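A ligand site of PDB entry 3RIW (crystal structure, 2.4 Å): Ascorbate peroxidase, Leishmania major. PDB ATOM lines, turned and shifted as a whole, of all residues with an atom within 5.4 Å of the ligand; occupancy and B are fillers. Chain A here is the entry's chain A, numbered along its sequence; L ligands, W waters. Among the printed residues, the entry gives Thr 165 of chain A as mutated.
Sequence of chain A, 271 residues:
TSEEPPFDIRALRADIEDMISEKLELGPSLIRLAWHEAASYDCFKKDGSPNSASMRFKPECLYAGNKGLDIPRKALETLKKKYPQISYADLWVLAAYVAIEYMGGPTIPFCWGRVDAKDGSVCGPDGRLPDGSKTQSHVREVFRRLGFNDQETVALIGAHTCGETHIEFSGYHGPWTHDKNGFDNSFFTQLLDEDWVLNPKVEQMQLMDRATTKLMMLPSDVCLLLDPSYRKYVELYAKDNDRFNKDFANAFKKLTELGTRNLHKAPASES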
ATOM      1  N   GLU A  25      32.306 -26.890  -6.903  1.00  0.00           N
ATOM      2  CA  GLU A  25      30.912 -26.506  -6.998  1.00  0.00           C
ATOM      3  C   GLU A  25      30.207 -27.158  -8.203  1.00  0.00           C
ATOM      4  O   GLU A  25      28.991 -27.207  -8.307  1.00  0.00           O
ATOM      5  CB  GLU A  25      30.811 -24.982  -7.055  1.00  0.00           C
ATOM      6  CG  GLU A  25      31.853 -24.357  -7.936  1.00  0.00           C
ATOM      7  CD  GLU A  25      33.177 -24.014  -7.218  1.00  0.00           C
ATOM      8  OE1 GLU A  25      33.874 -24.915  -6.712  1.00  0.00           O
ATOM      9  OE2 GLU A  25      33.521 -22.819  -7.199  1.00  0.00           O
ATOM     10  N   PRO A  28      27.765 -30.928  -7.579  1.00  0.00           N
ATOM     11  CA  PRO A  28      26.334 -30.790  -7.318  1.00  0.00           C
ATOM     12  C   PRO A  28      25.547 -30.221  -8.483  1.00  0.00           C
ATOM     13  O   PRO A  28      24.427 -30.672  -8.719  1.00  0.00           O
ATOM     14  CB  PRO A  28      26.275 -29.823  -6.130  1.00  0.00           C
ATOM     15  CG  PRO A  28      27.584 -30.077  -5.411  1.00  0.00           C
ATOM     16  CD  PRO A  28      28.566 -30.259  -6.530  1.00  0.00           C
ATOM     17  N   SER A  29      26.109 -29.288  -9.227  1.00  0.00           N
ATOM     18  CA  SER A  29      25.359 -28.758 -10.380  1.00  0.00           C
ATOM     19  C   SER A  29      25.100 -29.821 -11.452  1.00  0.00           C
ATOM     20  O   SER A  29      24.049 -29.831 -12.027  1.00  0.00           O
ATOM     21  CB  SER A  29      25.946 -27.466 -10.953  1.00  0.00           C
ATOM     22  OG  SER A  29      27.228 -27.703 -11.498  1.00  0.00           O
ATOM     23  N   ILE A  31      24.452 -32.888 -10.831  1.00  0.00           N
ATOM     24  CA  ILE A  31      23.309 -33.654 -10.319  1.00  0.00           C
ATOM     25  C   ILE A  31      22.004 -32.887 -10.579  1.00  0.00           C
ATOM     26  O   ILE A  31      21.012 -33.430 -11.060  1.00  0.00           O
ATOM     27  CB  ILE A  31      23.470 -33.974  -8.808  1.00  0.00           C
ATOM     28  CG1 ILE A  31      24.716 -34.875  -8.579  1.00  0.00           C
ATOM     29  CG2 ILE A  31      22.215 -34.599  -8.235  1.00  0.00           C
ATOM     30  CD1 ILE A  31      25.057 -35.027  -7.087  1.00  0.00           C
ATOM     31  N   ARG A  32      22.018 -31.593 -10.270  1.00  0.00           N
ATOM     32  CA  ARG A  32      20.894 -30.752 -10.540  1.00  0.00           C
ATOM     33  C   ARG A  32      20.599 -30.700 -12.063  1.00  0.00           C
ATOM     34  O   ARG A  32      19.436 -30.730 -12.463  1.00  0.00           O
ATOM     35  CB  ARG A  32      21.141 -29.370  -9.942  1.00  0.00           C
ATOM     36  CG  ARG A  32      19.985 -28.428 -10.148  1.00  0.00           C
ATOM     37  CD  ARG A  32      20.335 -27.011  -9.804  1.00  0.00           C
ATOM     38  NE  ARG A  32      19.259 -26.141 -10.230  1.00  0.00           N
ATOM     39  CZ  ARG A  32      19.418 -24.934 -10.768  1.00  0.00           C
ATOM     40  NH1 ARG A  32      20.612 -24.412 -10.957  1.00  0.00           N
ATOM     41  NH2 ARG A  32      18.358 -24.232 -11.112  1.00  0.00           N
ATOM     42  N   TRP A  35      18.823 -33.970 -12.997  1.00  0.00           N
ATOM     43  CA  TRP A  35      17.512 -34.039 -12.393  1.00  0.00           C
ATOM     44  C   TRP A  35      16.531 -33.179 -13.175  1.00  0.00           C
ATOM     45  O   TRP A  35      15.424 -33.621 -13.503  1.00  0.00           O
ATOM     46  CB  TRP A  35      17.602 -33.619 -10.937  1.00  0.00           C
ATOM     47  CG  TRP A  35      16.491 -32.827 -10.307  1.00  0.00           C
ATOM     48  CD1 TRP A  35      16.650 -31.626  -9.707  1.00  0.00           C
ATOM     49  CD2 TRP A  35      15.126 -33.189 -10.109  1.00  0.00           C
ATOM     50  NE1 TRP A  35      15.466 -31.200  -9.171  1.00  0.00           N
ATOM     51  CE2 TRP A  35      14.504 -32.130  -9.412  1.00  0.00           C
ATOM     52  CE3 TRP A  35      14.352 -34.303 -10.462  1.00  0.00           C
ATOM     53  CZ2 TRP A  35      13.136 -32.126  -9.054  1.00  0.00           C
ATOM     54  CZ3 TRP A  35      12.974 -34.321 -10.102  1.00  0.00           C
ATOM     55  CH2 TRP A  35      12.392 -33.231  -9.400  1.00  0.00           C
ATOM     56  N   LYS A  67      17.530 -21.875 -14.386  1.00  0.00           N
ATOM     57  CA  LYS A  67      18.523 -20.787 -14.341  1.00  0.00           C
ATOM     58  C   LYS A  67      19.837 -21.287 -13.676  1.00  0.00           C
ATOM     59  O   LYS A  67      19.842 -21.918 -12.611  1.00  0.00           O
ATOM     60  CB  LYS A  67      17.938 -19.592 -13.592  1.00  0.00           C
ATOM     61  CG  LYS A  67      18.550 -18.251 -13.975  1.00  0.00           C
ATOM     62  CD  LYS A  67      17.828 -17.057 -13.346  1.00  0.00           C
ATOM     63  CE  LYS A  67      18.609 -15.783 -13.704  1.00  0.00           C
ATOM     64  NZ  LYS A  67      18.353 -14.664 -12.747  1.00  0.00           N
ATOM     65  N   PRO A 130       9.730 -28.165  -9.785  1.00  0.00           N
ATOM     66  CA  PRO A 130       9.144 -27.795  -8.497  1.00  0.00           C
ATOM     67  C   PRO A 130       9.685 -26.462  -8.048  1.00  0.00           C
ATOM     68  O   PRO A 130      10.825 -26.161  -8.320  1.00  0.00           O
ATOM     69  CB  PRO A 130       9.619 -28.909  -7.545  1.00  0.00           C
ATOM     70  CG  PRO A 130      10.222 -29.954  -8.399  1.00  0.00           C
ATOM     71  CD  PRO A 130      10.700 -29.254  -9.660  1.00  0.00           C
ATOM     72  N   ASP A 131       8.868 -25.686  -7.342  1.00  0.00           N
ATOM     73  CA  ASP A 131       9.161 -24.334  -6.888  1.00  0.00           C
ATOM     74  C   ASP A 131       9.516 -24.440  -5.422  1.00  0.00           C
ATOM     75  O   ASP A 131       8.705 -24.927  -4.640  1.00  0.00           O
ATOM     76  CB  ASP A 131       7.867 -23.532  -6.997  1.00  0.00           C
ATOM     77  CG  ASP A 131       8.066 -22.033  -6.831  1.00  0.00           C
ATOM     78  OD1 ASP A 131       8.696 -21.543  -5.841  1.00  0.00           O
ATOM     79  OD2 ASP A 131       7.518 -21.330  -7.712  1.00  0.00           O
ATOM     80  N   GLY A 132      10.705 -23.956  -5.050  1.00  0.00           N
ATOM     81  CA  GLY A 132      11.166 -23.995  -3.655  1.00  0.00           C
ATOM     82  C   GLY A 132      10.243 -23.316  -2.674  1.00  0.00           C
ATOM     83  O   GLY A 132      10.303 -23.592  -1.477  1.00  0.00           O
ATOM     84  N   VAL A 139       4.617 -30.387  -4.028  1.00  0.00           N
ATOM     85  CA  VAL A 139       5.671 -31.364  -4.154  1.00  0.00           C
ATOM     86  C   VAL A 139       5.104 -32.745  -4.505  1.00  0.00           C
ATOM     87  O   VAL A 139       5.585 -33.397  -5.424  1.00  0.00           O
ATOM     88  CB  VAL A 139       6.485 -31.460  -2.841  1.00  0.00           C
ATOM     89  CG1 VAL A 139       7.395 -32.718  -2.814  1.00  0.00           C
ATOM     90  CG2 VAL A 139       7.283 -30.152  -2.589  1.00  0.00           C
ATOM     91  N   PHE A 143       5.902 -34.783  -8.035  1.00  0.00           N
ATOM     92  CA  PHE A 143       6.480 -36.121  -8.036  1.00  0.00           C
ATOM     93  C   PHE A 143       5.512 -37.235  -8.492  1.00  0.00           C
ATOM     94  O   PHE A 143       5.925 -38.193  -9.174  1.00  0.00           O
ATOM     95  CB  PHE A 143       7.154 -36.413  -6.721  1.00  0.00           C
ATOM     96  CG  PHE A 143       8.514 -35.751  -6.578  1.00  0.00           C
ATOM     97  CD1 PHE A 143       8.635 -34.432  -6.185  1.00  0.00           C
ATOM     98  CD2 PHE A 143       9.690 -36.463  -6.865  1.00  0.00           C
ATOM     99  CE1 PHE A 143       9.909 -33.832  -6.073  1.00  0.00           C
ATOM    100  CE2 PHE A 143      10.949 -35.875  -6.758  1.00  0.00           C
ATOM    101  CZ  PHE A 143      11.049 -34.547  -6.364  1.00  0.00           C
ATOM    102  N   LEU A 156      14.980 -38.856  -3.202  1.00  0.00           N
ATOM    103  CA  LEU A 156      15.445 -37.935  -4.194  1.00  0.00           C
ATOM    104  C   LEU A 156      15.780 -36.551  -3.630  1.00  0.00           C
ATOM    105  O   LEU A 156      16.833 -36.006  -3.942  1.00  0.00           O
ATOM    106  CB  LEU A 156      14.432 -37.807  -5.302  1.00  0.00           C
ATOM    107  CG  LEU A 156      14.442 -39.035  -6.214  1.00  0.00           C
ATOM    108  CD1 LEU A 156      13.333 -38.849  -7.247  1.00  0.00           C
ATOM    109  CD2 LEU A 156      15.787 -39.168  -6.897  1.00  0.00           C
ATOM    110  N   ILE A 157      14.901 -35.980  -2.800  1.00  0.00           N
ATOM    111  CA  ILE A 157      15.138 -34.620  -2.349  1.00  0.00           C
ATOM    112  C   ILE A 157      16.399 -34.587  -1.469  1.00  0.00           C
ATOM    113  O   ILE A 157      17.001 -33.539  -1.295  1.00  0.00           O
ATOM    114  CB  ILE A 157      13.910 -33.985  -1.648  1.00  0.00           C
ATOM    115  CG1 ILE A 157      12.790 -33.770  -2.671  1.00  0.00           C
ATOM    116  CG2 ILE A 157      14.291 -32.665  -1.048  1.00  0.00           C
ATOM    117  CD1 ILE A 157      11.420 -33.659  -2.126  1.00  0.00           C
ATOM    118  N   ALA A 159      19.208 -35.372  -2.176  1.00  0.00           N
ATOM    119  CA  ALA A 159      20.358 -34.910  -2.955  1.00  0.00           C
ATOM    120  C   ALA A 159      20.752 -33.541  -2.454  1.00  0.00           C
ATOM    121  O   ALA A 159      21.873 -33.055  -2.727  1.00  0.00           O
ATOM    122  CB  ALA A 159      20.026 -34.840  -4.411  1.00  0.00           C
ATOM    123  N   HIS A 160      19.858 -32.893  -1.705  1.00  0.00           N
ATOM    124  CA  HIS A 160      20.207 -31.572  -1.162  1.00  0.00           C
ATOM    125  C   HIS A 160      21.260 -31.684  -0.087  1.00  0.00           C
ATOM    126  O   HIS A 160      21.693 -30.677   0.503  1.00  0.00           O
ATOM    127  CB  HIS A 160      18.985 -30.777  -0.733  1.00  0.00           C
ATOM    128  CG  HIS A 160      18.202 -30.230  -1.905  1.00  0.00           C
ATOM    129  ND1 HIS A 160      16.941 -29.679  -1.769  1.00  0.00           N
ATOM    130  CD2 HIS A 160      18.512 -30.119  -3.220  1.00  0.00           C
ATOM    131  CE1 HIS A 160      16.511 -29.273  -2.956  1.00  0.00           C
ATOM    132  NE2 HIS A 160      17.443 -29.531  -3.851  1.00  0.00           N
ATOM    133  N   CYS A 162      24.135 -32.121  -0.899  1.00  0.00           N
ATOM    134  CA  CYS A 162      25.324 -31.511  -1.473  1.00  0.00           C
ATOM    135  C   CYS A 162      24.961 -30.229  -2.216  1.00  0.00           C
ATOM    136  O   CYS A 162      23.821 -30.063  -2.684  1.00  0.00           O
ATOM    137  CB  CYS A 162      26.073 -32.501  -2.378  1.00  0.00           C
ATOM    138  SG  CYS A 162      25.158 -32.949  -3.850  1.00  0.00           S
ATOM    139  N   GLY A 163      25.923 -29.330  -2.348  1.00  0.00           N
ATOM    140  CA  GLY A 163      25.689 -28.099  -3.096  1.00  0.00           C
ATOM    141  C   GLY A 163      24.976 -27.039  -2.290  1.00  0.00           C
ATOM    142  O   GLY A 163      24.904 -27.117  -1.057  1.00  0.00           O
ATOM    143  N   GLU A 164      24.444 -26.044  -2.981  1.00  0.00           N
ATOM    144  CA  GLU A 164      23.934 -24.862  -2.346  1.00  0.00           C
ATOM    145  C   GLU A 164      23.023 -24.070  -3.295  1.00  0.00           C
ATOM    146  O   GLU A 164      22.992 -24.335  -4.510  1.00  0.00           O
ATOM    147  CB  GLU A 164      25.113 -23.980  -1.856  1.00  0.00           C
ATOM    148  CG  GLU A 164      25.913 -23.325  -2.952  1.00  0.00           C
ATOM    149  CD  GLU A 164      27.241 -22.753  -2.429  1.00  0.00           C
ATOM    150  OE1 GLU A 164      28.310 -23.139  -2.973  1.00  0.00           O
ATOM    151  OE2 GLU A 164      27.243 -21.950  -1.474  1.00  0.00           O
ATOM    152  N   THR A 165      22.279 -23.118  -2.722  1.00  0.00           N
ATOM    153  CA  THR A 165      21.460 -22.223  -3.528  1.00  0.00           C
ATOM    154  C   THR A 165      22.268 -20.965  -3.889  1.00  0.00           C
ATOM    155  O   THR A 165      23.216 -20.610  -3.192  1.00  0.00           O
ATOM    156  CB  THR A 165      20.136 -21.871  -2.809  1.00  0.00           C
ATOM    157  OG1 THR A 165      20.424 -21.270  -1.557  1.00  0.00           O
ATOM    158  CG2 THR A 165      19.310 -23.135  -2.527  1.00  0.00           C
ATOM    159  N   HIS A 166      21.910 -20.310  -4.992  1.00  0.00           N
ATOM    160  CA  HIS A 166      22.615 -19.095  -5.410  1.00  0.00           C
ATOM    161  C   HIS A 166      21.580 -18.010  -5.670  1.00  0.00           C
ATOM    162  O   HIS A 166      20.546 -18.285  -6.294  1.00  0.00           O
ATOM    163  CB  HIS A 166      23.456 -19.368  -6.671  1.00  0.00           C
ATOM    164  CG  HIS A 166      24.325 -20.575  -6.565  1.00  0.00           C
ATOM    165  ND1 HIS A 166      23.866 -21.857  -6.808  1.00  0.00           N
ATOM    166  CD2 HIS A 166      25.627 -20.704  -6.229  1.00  0.00           C
ATOM    167  CE1 HIS A 166      24.849 -22.715  -6.611  1.00  0.00           C
ATOM    168  NE2 HIS A 166      25.935 -22.046  -6.258  1.00  0.00           N
ATOM    169  N   ILE A 167      21.832 -16.797  -5.174  1.00  0.00           N
ATOM    170  CA  ILE A 167      20.868 -15.716  -5.301  1.00  0.00           C
ATOM    171  C   ILE A 167      20.618 -15.469  -6.772  1.00  0.00           C
ATOM    172  O   ILE A 167      19.487 -15.392  -7.228  1.00  0.00           O
ATOM    173  CB  ILE A 167      21.347 -14.400  -4.640  1.00  0.00           C
ATOM    174  CG1 ILE A 167      21.676 -14.594  -3.175  1.00  0.00           C
ATOM    175  CG2 ILE A 167      20.259 -13.289  -4.769  1.00  0.00           C
ATOM    176  CD1 ILE A 167      20.597 -14.122  -2.197  1.00  0.00           C
ATOM    177  N   PHE A 169      20.662 -17.439  -9.190  1.00  0.00           N
ATOM    178  CA  PHE A 169      19.912 -18.503  -9.895  1.00  0.00           C
ATOM    179  C   PHE A 169      18.475 -18.716  -9.439  1.00  0.00           C
ATOM    180  O   PHE A 169      17.538 -18.712 -10.253  1.00  0.00           O
ATOM    181  CB  PHE A 169      20.678 -19.852  -9.967  1.00  0.00           C
ATOM    182  CG  PHE A 169      22.064 -19.743 -10.539  1.00  0.00           C
ATOM    183  CD1 PHE A 169      22.394 -18.743 -11.453  1.00  0.00           C
ATOM    184  CD2 PHE A 169      23.033 -20.645 -10.178  1.00  0.00           C
ATOM    185  CE1 PHE A 169      23.669 -18.636 -11.962  1.00  0.00           C
ATOM    186  CE2 PHE A 169      24.314 -20.546 -10.689  1.00  0.00           C
ATOM    187  CZ  PHE A 169      24.629 -19.538 -11.580  1.00  0.00           C
ATOM    188  N   SER A 170      18.282 -18.926  -8.137  1.00  0.00           N
ATOM    189  CA  SER A 170      16.979 -19.225  -7.591  1.00  0.00           C
ATOM    190  C   SER A 170      16.502 -18.042  -6.761  1.00  0.00           C
ATOM    191  O   SER A 170      15.340 -17.963  -6.442  1.00  0.00           O
ATOM    192  CB  SER A 170      17.084 -20.440  -6.658  1.00  0.00           C
ATOM    193  OG  SER A 170      18.219 -20.333  -5.796  1.00  0.00           O
ATOM    194  N   GLY A 171      17.409 -17.147  -6.367  1.00  0.00           N
ATOM    195  CA  GLY A 171      17.053 -16.129  -5.393  1.00  0.00           C
ATOM    196  C   GLY A 171      17.156 -16.575  -3.932  1.00  0.00           C
ATOM    197  O   GLY A 171      16.905 -15.813  -3.016  1.00  0.00           O
ATOM    198  N   TYR A 172      17.528 -17.827  -3.710  1.00  0.00           N
ATOM    199  CA  TYR A 172      17.810 -18.316  -2.375  1.00  0.00           C
ATOM    200  C   TYR A 172      19.305 -18.275  -2.172  1.00  0.00           C
ATOM    201  O   TYR A 172      20.062 -18.216  -3.153  1.00  0.00           O
ATOM    202  CB  TYR A 172      17.328 -19.743  -2.255  1.00  0.00           C
ATOM    203  CG  TYR A 172      15.843 -19.867  -2.316  1.00  0.00           C
ATOM    204  CD1 TYR A 172      15.022 -19.423  -1.280  1.00  0.00           C
ATOM    205  CD2 TYR A 172      15.234 -20.453  -3.424  1.00  0.00           C
ATOM    206  CE1 TYR A 172      13.650 -19.560  -1.345  1.00  0.00           C
ATOM    207  CE2 TYR A 172      13.844 -20.617  -3.489  1.00  0.00           C
ATOM    208  CZ  TYR A 172      13.068 -20.162  -2.456  1.00  0.00           C
ATOM    209  OH  TYR A 172      11.703 -20.303  -2.532  1.00  0.00           O
ATOM    210  N   TRP A 176      22.630 -26.413   2.443  1.00  0.00           N
ATOM    211  CA  TRP A 176      21.738 -27.072   3.369  1.00  0.00           C
ATOM    212  C   TRP A 176      22.528 -27.751   4.463  1.00  0.00           C
ATOM    213  O   TRP A 176      21.971 -28.052   5.527  1.00  0.00           O
ATOM    214  CB  TRP A 176      20.932 -28.186   2.673  1.00  0.00           C
ATOM    215  CG  TRP A 176      19.942 -27.737   1.670  1.00  0.00           C
ATOM    216  CD1 TRP A 176      18.603 -27.513   1.896  1.00  0.00           C
ATOM    217  CD2 TRP A 176      20.169 -27.473   0.273  1.00  0.00           C
ATOM    218  NE1 TRP A 176      17.984 -27.135   0.723  1.00  0.00           N
ATOM    219  CE2 TRP A 176      18.917 -27.106  -0.294  1.00  0.00           C
ATOM    220  CE3 TRP A 176      21.301 -27.543  -0.557  1.00  0.00           C
ATOM    221  CZ2 TRP A 176      18.771 -26.790  -1.656  1.00  0.00           C
ATOM    222  CZ3 TRP A 176      21.149 -27.205  -1.912  1.00  0.00           C
ATOM    223  CH2 TRP A 176      19.897 -26.836  -2.446  1.00  0.00           C
ATOM    224  N   LEU A 218      14.751 -24.656   2.297  1.00  0.00           N
ATOM    225  CA  LEU A 218      13.655 -24.040   1.577  1.00  0.00           C
ATOM    226  C   LEU A 218      12.335 -24.432   2.216  1.00  0.00           C
ATOM    227  O   LEU A 218      12.288 -25.430   2.912  1.00  0.00           O
ATOM    228  CB  LEU A 218      13.635 -24.513   0.140  1.00  0.00           C
ATOM    229  CG  LEU A 218      14.911 -24.236  -0.649  1.00  0.00           C
ATOM    230  CD1 LEU A 218      14.930 -25.025  -1.981  1.00  0.00           C
ATOM    231  CD2 LEU A 218      15.015 -22.809  -0.901  1.00  0.00           C
ATOM    232  N   SER A 220      10.067 -25.868   0.603  1.00  0.00           N
ATOM    233  CA  SER A 220       9.829 -27.204   0.065  1.00  0.00           C
ATOM    234  C   SER A 220      10.594 -28.314   0.812  1.00  0.00           C
ATOM    235  O   SER A 220      10.206 -29.480   0.746  1.00  0.00           O
ATOM    236  CB  SER A 220      10.129 -27.228  -1.416  1.00  0.00           C
ATOM    237  OG  SER A 220      11.432 -26.691  -1.621  1.00  0.00           O
ATOM    238  N   PHE A 248      18.261 -43.988  -2.684  1.00  0.00           N
ATOM    239  CA  PHE A 248      18.594 -42.882  -3.538  1.00  0.00           C
ATOM    240  C   PHE A 248      19.073 -43.389  -4.896  1.00  0.00           C
ATOM    241  O   PHE A 248      18.621 -42.937  -5.930  1.00  0.00           O
ATOM    242  CB  PHE A 248      19.657 -41.932  -2.971  1.00  0.00           C
ATOM    243  CG  PHE A 248      19.947 -40.810  -3.920  1.00  0.00           C
ATOM    244  CD1 PHE A 248      19.167 -39.633  -3.889  1.00  0.00           C
ATOM    245  CD2 PHE A 248      20.914 -40.947  -4.908  1.00  0.00           C
ATOM    246  CE1 PHE A 248      19.384 -38.575  -4.825  1.00  0.00           C
ATOM    247  CE2 PHE A 248      21.124 -39.901  -5.870  1.00  0.00           C
ATOM    248  CZ  PHE A 248      20.373 -38.715  -5.833  1.00  0.00           C
ATOM    249  N   PHE A 252      17.191 -42.421  -8.220  1.00  0.00           N
ATOM    250  CA  PHE A 252      17.896 -41.623  -9.200  1.00  0.00           C
ATOM    251  C   PHE A 252      18.035 -42.319 -10.551  1.00  0.00           C
ATOM    252  O   PHE A 252      17.908 -41.688 -11.597  1.00  0.00           O
ATOM    253  CB  PHE A 252      19.237 -41.119  -8.679  1.00  0.00           C
ATOM    254  CG  PHE A 252      19.743 -39.906  -9.404  1.00  0.00           C
ATOM    255  CD1 PHE A 252      19.163 -38.664  -9.202  1.00  0.00           C
ATOM    256  CD2 PHE A 252      20.769 -40.002 -10.318  1.00  0.00           C
ATOM    257  CE1 PHE A 252      19.634 -37.530  -9.885  1.00  0.00           C
ATOM    258  CE2 PHE A 252      21.223 -38.886 -10.987  1.00  0.00           C
ATOM    259  CZ  PHE A 252      20.662 -37.656 -10.777  1.00  0.00           C
ATOM    260  N   LEU A 255      14.784 -42.300 -12.171  1.00  0.00           N
ATOM    261  CA  LEU A 255      14.513 -40.915 -12.624  1.00  0.00           C
ATOM    262  C   LEU A 255      15.228 -40.599 -13.944  1.00  0.00           C
ATOM    263  O   LEU A 255      14.666 -40.019 -14.859  1.00  0.00           O
ATOM    264  CB  LEU A 255      14.957 -39.914 -11.545  1.00  0.00           C
ATOM    265  CG  LEU A 255      15.099 -38.479 -11.993  1.00  0.00           C
ATOM    266  CD1 LEU A 255      13.738 -37.824 -12.011  1.00  0.00           C
ATOM    267  CD2 LEU A 255      15.973 -37.720 -11.011  1.00  0.00           C
HETATM  268  C1  LIG L   1      19.679 -26.956  -5.972  1.00  0.00           C
HETATM  269  C2  LIG L   1      14.875 -26.654  -5.363  1.00  0.00           C
HETATM  270  C3  LIG L   1      14.536 -31.465  -5.723  1.00  0.00           C
HETATM  271  C4  LIG L   1      19.238 -31.718  -6.580  1.00  0.00           C
HETATM  272  C5  LIG L   1      18.406 -26.431  -5.825  1.00  0.00           C
HETATM  273  C6  LIG L   1      18.053 -25.033  -5.748  1.00  0.00           C
HETATM  274  C7  LIG L   1      16.723 -24.978  -5.560  1.00  0.00           C
HETATM  275  C8  LIG L   1      16.208 -26.302  -5.525  1.00  0.00           C
HETATM  276  C9  LIG L   1      15.801 -23.744  -5.395  1.00  0.00           C
HETATM  277  C10 LIG L   1      19.071 -23.863  -5.832  1.00  0.00           C
HETATM  278  C11 LIG L   1      19.512 -23.620  -7.280  1.00  0.00           C
HETATM  279  C12 LIG L   1      20.597 -22.567  -7.313  1.00  0.00           C
HETATM  280  O1  LIG L   1      20.402 -21.426  -6.790  1.00  0.00           O
HETATM  281  O2  LIG L   1      21.684 -22.879  -7.882  1.00  0.00           O
HETATM  282  C13 LIG L   1      14.383 -27.940  -5.397  1.00  0.00           C
HETATM  283  C14 LIG L   1      13.000 -28.292  -5.241  1.00  0.00           C
HETATM  284  C15 LIG L   1      12.930 -29.607  -5.350  1.00  0.00           C
HETATM  285  C16 LIG L   1      14.235 -30.135  -5.580  1.00  0.00           C
HETATM  286  C17 LIG L   1      11.827 -27.300  -4.994  1.00  0.00           C
HETATM  287  C18 LIG L   1      11.682 -30.457  -5.240  1.00  0.00           C
HETATM  288  C19 LIG L   1      10.992 -30.385  -4.099  1.00  0.00           C
HETATM  289  C20 LIG L   1      15.750 -31.926  -6.088  1.00  0.00           C
HETATM  290  C21 LIG L   1      16.046 -33.284  -6.486  1.00  0.00           C
HETATM  291  C22 LIG L   1      17.358 -33.346  -6.752  1.00  0.00           C
HETATM  292  C23 LIG L   1      17.912 -32.033  -6.479  1.00  0.00           C
HETATM  293  C24 LIG L   1      14.995 -34.408  -6.623  1.00  0.00           C
HETATM  294  C25 LIG L   1      18.217 -34.529  -7.247  1.00  0.00           C
HETATM  295  C26 LIG L   1      17.893 -35.792  -7.001  1.00  0.00           C
HETATM  296  C27 LIG L   1      19.830 -30.517  -6.364  1.00  0.00           C
HETATM  297  C28 LIG L   1      21.267 -30.289  -6.197  1.00  0.00           C
HETATM  298  C29 LIG L   1      21.408 -28.789  -6.015  1.00  0.00           C
HETATM  299  C30 LIG L   1      20.029 -28.283  -6.076  1.00  0.00           C
HETATM  300  C31 LIG L   1      22.369 -31.357  -6.233  1.00  0.00           C
HETATM  301  C32 LIG L   1      22.671 -27.964  -5.792  1.00  0.00           C
HETATM  302  C33 LIG L   1      23.056 -27.355  -7.147  1.00  0.00           C
HETATM  303  C34 LIG L   1      24.367 -26.561  -7.101  1.00  0.00           C
HETATM  304  O3  LIG L   1      24.681 -26.006  -8.184  1.00  0.00           O
HETATM  305  O4  LIG L   1      25.115 -26.451  -6.063  1.00  0.00           O
HETATM  306  N1  LIG L   1      17.256 -27.174  -5.667  1.00  0.00           N
HETATM  307  N2  LIG L   1      15.115 -29.105  -5.568  1.00  0.00           N
HETATM  308  N3  LIG L   1      16.917 -31.194  -6.056  1.00  0.00           N
HETATM  309  N4  LIG L   1      19.145 -29.341  -6.238  1.00  0.00           N
HETATM  310 FE1  LIG L   1      17.109 -29.244  -5.817  1.00  0.00          FE
HETATM  311  O   HOH W   1      27.817 -26.045  -6.018  1.00  0.00           O
HETATM  312  O   HOH W   2      13.974 -28.115  -8.524  1.00  0.00           O
HETATM  313  O   HOH W   3      16.501 -26.040  -8.950  1.00  0.00           O
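The backbone carbonyl oxygen (O) of His 166 is in hydrogen-bond range of the side-chain hydroxyl (OG) of Ser 170 (3.1 Å).
OG of Ser 170 sits close to N of Tyr 172, 3.3 Å away.
The backbone carbonyl oxygen (O) of Tyr 172 lies within hydrogen-bond range of the backbone NH (N) of Ile 167, at 3.0 Å.
The side-chain sulfur (SG) of Cys 162 sits at hydrogen-bond distance from the backbone carbonyl oxygen (O) of Ala 159.
O of Tyr 172 lies close to N of His 166 (3.3 Å).
The backbone NH (N) of Ser 220 sits at hydrogen-bond distance from the backbone carbonyl oxygen (O) of Gly 132 (3.1 Å).
A ring nitrogen (ND1) of His 166 sits close to the backbone carbonyl oxygen (O) of Glu 164, at 3.5 Å.
The backbone NH of Gly 171 lies within hydrogen-bond range of the backbone carbonyl oxygen of His 166 (3.3 Å).
Water W1 lies within hydrogen-bond range of an oxygen (O4) of the ligand (2.7 Å) and the backbone carbonyl oxygen of Glu 25 (2.8 Å).
A ring nitrogen (NE2) of His 160 binds an iron atom (FE1) of the ligand.
The side-chain hydroxyl of Ser 170 sits at hydrogen-bond distance from an oxygen (O1) of the ligand.
The backbone NH (N) of Glu 164 is in hydrogen-bond range of an oxygen (O4) of the ligand (3.2 Å).
A ring nitrogen (ND1) of His 166 lies within hydrogen-bond range of an oxygen (O2) of the ligand (2.6 Å).
The backbone NH of His 166 is in hydrogen-bond range of an oxygen (O1) of the ligand, at 2.6 Å.
The guanidinium group (NH1) of Arg 32 is in salt-bridge range of an oxygen (O2) of the ligand.
The indole nitrogen (NE1) of Trp 35 lies close to a nitrogen (N3) of the ligand.
Pro 28 touches the ligand.
Ser 29 touches the ligand (CB to O3, 3.4 Å).
Ile 31 touches the ligand.
CB of Pro 130 touches C18 of the ligand, 3.5 Å away.
Asp 131 touches the ligand (C to C17, 3.7 Å).
Gly 132 touches the ligand.
CE1 of Phe 143 touches C18 of the ligand, 3.9 Å away.
Leu 156 touches the ligand (O to C26, 3.2 Å).
Ile 157 touches the ligand (CD1 to C19, 3.8 Å).
CB of Ala 159 touches C25 of the ligand, at 3.4 Å.
Cys 162 touches the ligand (O to C32, 3.9 Å).
CA of Gly 163 touches O4 of the ligand (3.4 Å).
Thr 165 touches the ligand (CG2 to C10, 3.4 Å).
Phe 169 touches the ligand (CD2 to O2, 3.5 Å).
Tyr 172 touches the ligand.
CH2 of Trp 176 touches C1 of the ligand (3.5 Å).
CD1 of Leu 218 touches C9 of the ligand, 3.7 Å away.
Ser 220 touches the ligand (OG to C17, 3.5 Å).
Phe 248 touches the ligand.
Phe 252 touches the ligand.
The nearest printed residue that does not touch the ligand is Val 139 (4.01 Å).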
